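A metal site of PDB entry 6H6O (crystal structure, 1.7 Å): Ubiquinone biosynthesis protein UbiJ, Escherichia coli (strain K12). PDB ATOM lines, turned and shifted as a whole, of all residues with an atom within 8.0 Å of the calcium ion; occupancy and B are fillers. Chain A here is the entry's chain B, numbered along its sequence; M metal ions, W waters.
Water W1 lies within hydrogen-bond range of O of Arg 93 (2.7 Å) and OE2 of Glu 127 (2.8 Å).
The backbone NH (N) of Arg 95 is in hydrogen-bond range of the side-chain carboxylate (OD2) of Asp 124, 3.3 Å away. The guanidinium group (NH2) of Arg 93 lies within salt-bridge range of the side-chain carboxylate (OE1) of Glu 127 (2.8 Å).
Three residues have an atom within 4 Å of the calcium ion: Asp 124, Glu 127 and Asp 129.
The calcium ion is bound by the backbone carbonyl oxygen of Asp 124 (2.3 Å), the backbone carbonyl oxygen of Glu 127 (2.3 Å), water W1 (2.3 Å), the side-chain carboxylate of Asp 124 (2.4 Å) and the side-chain carboxylate of Asp 129 (2.5 Å). The calcium ion has five donor atoms within binding distance.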
ATOM      1  N   PHE A  29       7.216  25.051   9.581  1.00  0.00           N
ATOM      2  CA  PHE A  29       6.752  24.550  10.874  1.00  0.00           C
ATOM      3  C   PHE A  29       5.621  23.486  10.750  1.00  0.00           C
ATOM      4  O   PHE A  29       5.695  22.447  11.422  1.00  0.00           O
ATOM      5  CB  PHE A  29       6.328  25.719  11.779  1.00  0.00           C
ATOM      6  CG  PHE A  29       5.925  25.348  13.197  1.00  0.00           C
ATOM      7  CD1 PHE A  29       6.832  24.776  14.073  1.00  0.00           C
ATOM      8  CD2 PHE A  29       4.634  25.614  13.652  1.00  0.00           C
ATOM      9  CE1 PHE A  29       6.459  24.461  15.390  1.00  0.00           C
ATOM     10  CE2 PHE A  29       4.248  25.255  14.961  1.00  0.00           C
ATOM     11  CZ  PHE A  29       5.174  24.704  15.822  1.00  0.00           C
ATOM     12  N   ARG A  93       0.021  27.105  20.277  1.00  0.00           N
ATOM     13  CA  ARG A  93       0.569  25.772  19.944  1.00  0.00           C
ATOM     14  C   ARG A  93       0.221  24.769  21.061  1.00  0.00           C
ATOM     15  O   ARG A  93       0.868  23.724  21.195  1.00  0.00           O
ATOM     16  CB  ARG A  93       2.082  25.829  19.701  1.00  0.00           C
ATOM     17  CG  ARG A  93       2.523  26.801  18.603  1.00  0.00           C
ATOM     18  CD  ARG A  93       3.408  27.875  19.199  1.00  0.00           C
ATOM     19  NE  ARG A  93       4.731  27.355  19.565  1.00  0.00           N
ATOM     20  CZ  ARG A  93       5.606  28.014  20.315  1.00  0.00           C
ATOM     21  NH1 ARG A  93       5.310  29.201  20.820  1.00  0.00           N
ATOM     22  NH2 ARG A  93       6.783  27.470  20.593  1.00  0.00           N
ATOM     23  N   ASP A  94      -0.802  25.084  21.862  1.00  0.00           N
ATOM     24  CA  ASP A  94      -1.259  24.223  22.948  1.00  0.00           C
ATOM     25  C   ASP A  94      -2.789  24.172  22.908  1.00  0.00           C
ATOM     26  O   ASP A  94      -3.459  25.138  23.260  1.00  0.00           O
ATOM     27  CB  ASP A  94      -0.714  24.736  24.306  1.00  0.00           C
ATOM     28  CG  ASP A  94      -1.049  23.892  25.528  1.00  0.00           C
ATOM     29  OD1 ASP A  94      -1.538  22.753  25.352  1.00  0.00           O
ATOM     30  OD2 ASP A  94      -0.789  24.362  26.664  1.00  0.00           O
ATOM     31  N   ARG A  95      -3.332  23.039  22.429  1.00  0.00           N
ATOM     32  CA  ARG A  95      -4.774  22.883  22.254  1.00  0.00           C
ATOM     33  C   ARG A  95      -5.585  22.954  23.535  1.00  0.00           C
ATOM     34  O   ARG A  95      -6.717  23.430  23.505  1.00  0.00           O
ATOM     35  CB  ARG A  95      -5.150  21.612  21.466  1.00  0.00           C
ATOM     36  CG  ARG A  95      -6.299  21.889  20.498  1.00  0.00           C
ATOM     37  CD  ARG A  95      -7.410  20.853  20.483  1.00  0.00           C
ATOM     38  NE  ARG A  95      -8.191  20.973  19.252  1.00  0.00           N
ATOM     39  CZ  ARG A  95      -8.983  20.038  18.755  1.00  0.00           C
ATOM     40  NH1 ARG A  95      -9.145  18.888  19.395  1.00  0.00           N
ATOM     41  NH2 ARG A  95      -9.624  20.232  17.611  1.00  0.00           N
ATOM     42  N   VAL A 120      -4.665  25.207  16.108  1.00  0.00           N
ATOM     43  CA  VAL A 120      -3.945  25.037  17.374  1.00  0.00           C
ATOM     44  C   VAL A 120      -3.604  23.555  17.590  1.00  0.00           C
ATOM     45  O   VAL A 120      -2.467  23.246  17.938  1.00  0.00           O
ATOM     46  CB  VAL A 120      -4.701  25.675  18.562  1.00  0.00           C
ATOM     47  CG1 VAL A 120      -3.996  25.389  19.880  1.00  0.00           C
ATOM     48  CG2 VAL A 120      -4.832  27.186  18.376  1.00  0.00           C
ATOM     49  N   ALA A 121      -4.541  22.624  17.294  1.00  0.00           N
ATOM     50  CA  ALA A 121      -4.304  21.180  17.393  1.00  0.00           C
ATOM     51  C   ALA A 121      -3.156  20.786  16.452  1.00  0.00           C
ATOM     52  O   ALA A 121      -2.253  20.072  16.875  1.00  0.00           O
ATOM     53  CB  ALA A 121      -5.584  20.421  17.026  1.00  0.00           C
ATOM     54  N   LEU A 122      -3.150  21.329  15.189  1.00  0.00           N
ATOM     55  CA  LEU A 122      -2.097  21.057  14.216  1.00  0.00           C
ATOM     56  C   LEU A 122      -0.749  21.611  14.710  1.00  0.00           C
ATOM     57  O   LEU A 122       0.257  20.887  14.685  1.00  0.00           O
ATOM     58  CB  LEU A 122      -2.464  21.622  12.820  1.00  0.00           C
ATOM     59  CG  LEU A 122      -1.339  21.670  11.787  1.00  0.00           C
ATOM     60  CD1 LEU A 122      -0.787  20.250  11.451  1.00  0.00           C
ATOM     61  CD2 LEU A 122      -1.786  22.420  10.530  1.00  0.00           C
ATOM     62  N   ALA A 123      -0.743  22.897  15.144  1.00  0.00           N
ATOM     63  CA  ALA A 123       0.452  23.553  15.697  1.00  0.00           C
ATOM     64  C   ALA A 123       1.019  22.750  16.918  1.00  0.00           C
ATOM     65  O   ALA A 123       2.245  22.572  17.027  1.00  0.00           O
ATOM     66  CB  ALA A 123       0.103  24.980  16.093  1.00  0.00           C
ATOM     67  N   ASP A 124       0.149  22.208  17.773  1.00  0.00           N
ATOM     68  CA  ASP A 124       0.542  21.376  18.917  1.00  0.00           C
ATOM     69  C   ASP A 124       1.212  20.086  18.452  1.00  0.00           C
ATOM     70  O   ASP A 124       2.305  19.759  18.919  1.00  0.00           O
ATOM     71  CB  ASP A 124      -0.672  21.071  19.792  1.00  0.00           C
ATOM     72  CG  ASP A 124      -0.380  20.611  21.204  1.00  0.00           C
ATOM     73  OD1 ASP A 124       0.823  20.433  21.551  1.00  0.00           O
ATOM     74  OD2 ASP A 124      -1.342  20.457  21.979  1.00  0.00           O
ATOM     75  N   LEU A 125       0.612  19.405  17.447  1.00  0.00           N
ATOM     76  CA  LEU A 125       1.160  18.169  16.883  1.00  0.00           C
ATOM     77  C   LEU A 125       2.462  18.420  16.124  1.00  0.00           C
ATOM     78  O   LEU A 125       3.332  17.539  16.119  1.00  0.00           O
ATOM     79  CB  LEU A 125       0.131  17.462  15.995  1.00  0.00           C
ATOM     80  CG  LEU A 125      -1.052  16.837  16.783  1.00  0.00           C
ATOM     81  CD1 LEU A 125      -2.130  16.340  15.846  1.00  0.00           C
ATOM     82  CD2 LEU A 125      -0.586  15.704  17.750  1.00  0.00           C
ATOM     83  N   ALA A 126       2.624  19.614  15.545  1.00  0.00           N
ATOM     84  CA  ALA A 126       3.864  19.972  14.830  1.00  0.00           C
ATOM     85  C   ALA A 126       5.067  20.163  15.759  1.00  0.00           C
ATOM     86  O   ALA A 126       6.198  20.217  15.265  1.00  0.00           O
ATOM     87  CB  ALA A 126       3.631  21.257  14.038  1.00  0.00           C
ATOM     88  N   GLU A 127       4.875  20.242  17.090  1.00  0.00           N
ATOM     89  CA  GLU A 127       5.983  20.554  17.986  1.00  0.00           C
ATOM     90  C   GLU A 127       6.099  19.697  19.245  1.00  0.00           C
ATOM     91  O   GLU A 127       5.128  19.535  19.985  1.00  0.00           O
ATOM     92  CB  GLU A 127       5.824  22.040  18.367  1.00  0.00           C
ATOM     93  CG  GLU A 127       6.753  22.611  19.423  1.00  0.00           C
ATOM     94  CD  GLU A 127       6.362  24.035  19.748  1.00  0.00           C
ATOM     95  OE1 GLU A 127       7.122  24.958  19.374  1.00  0.00           O
ATOM     96  OE2 GLU A 127       5.256  24.247  20.298  1.00  0.00           O
ATOM     97  N   PHE A 128       7.321  19.192  19.501  1.00  0.00           N
ATOM     98  CA  PHE A 128       7.641  18.451  20.725  1.00  0.00           C
ATOM     99  C   PHE A 128       7.669  19.504  21.854  1.00  0.00           C
ATOM    100  O   PHE A 128       8.234  20.579  21.653  1.00  0.00           O
ATOM    101  CB  PHE A 128       9.040  17.782  20.607  1.00  0.00           C
ATOM    102  CG  PHE A 128       9.062  16.496  19.807  1.00  0.00           C
ATOM    103  CD1 PHE A 128       8.643  15.293  20.375  1.00  0.00           C
ATOM    104  CD2 PHE A 128       9.528  16.491  18.496  1.00  0.00           C
ATOM    105  CE1 PHE A 128       8.676  14.105  19.634  1.00  0.00           C
ATOM    106  CE2 PHE A 128       9.562  15.303  17.754  1.00  0.00           C
ATOM    107  CZ  PHE A 128       9.123  14.125  18.330  1.00  0.00           C
ATOM    108  N   ASP A 129       7.011  19.222  23.001  1.00  0.00           N
ATOM    109  CA  ASP A 129       6.919  20.161  24.129  1.00  0.00           C
ATOM    110  C   ASP A 129       8.241  20.332  24.879  1.00  0.00           C
ATOM    111  O   ASP A 129       9.103  19.448  24.853  1.00  0.00           O
ATOM    112  CB  ASP A 129       5.799  19.742  25.093  1.00  0.00           C
ATOM    113  CG  ASP A 129       4.374  19.917  24.567  1.00  0.00           C
ATOM    114  OD1 ASP A 129       4.195  20.083  23.337  1.00  0.00           O
ATOM    115  OD2 ASP A 129       3.442  19.848  25.395  1.00  0.00           O
HETATM  116 CA    CA M   1       3.143  20.136  21.052  1.00  0.00          CA
HETATM  117  O   HOH W   1       3.280  22.468  21.185  1.00  0.00           O
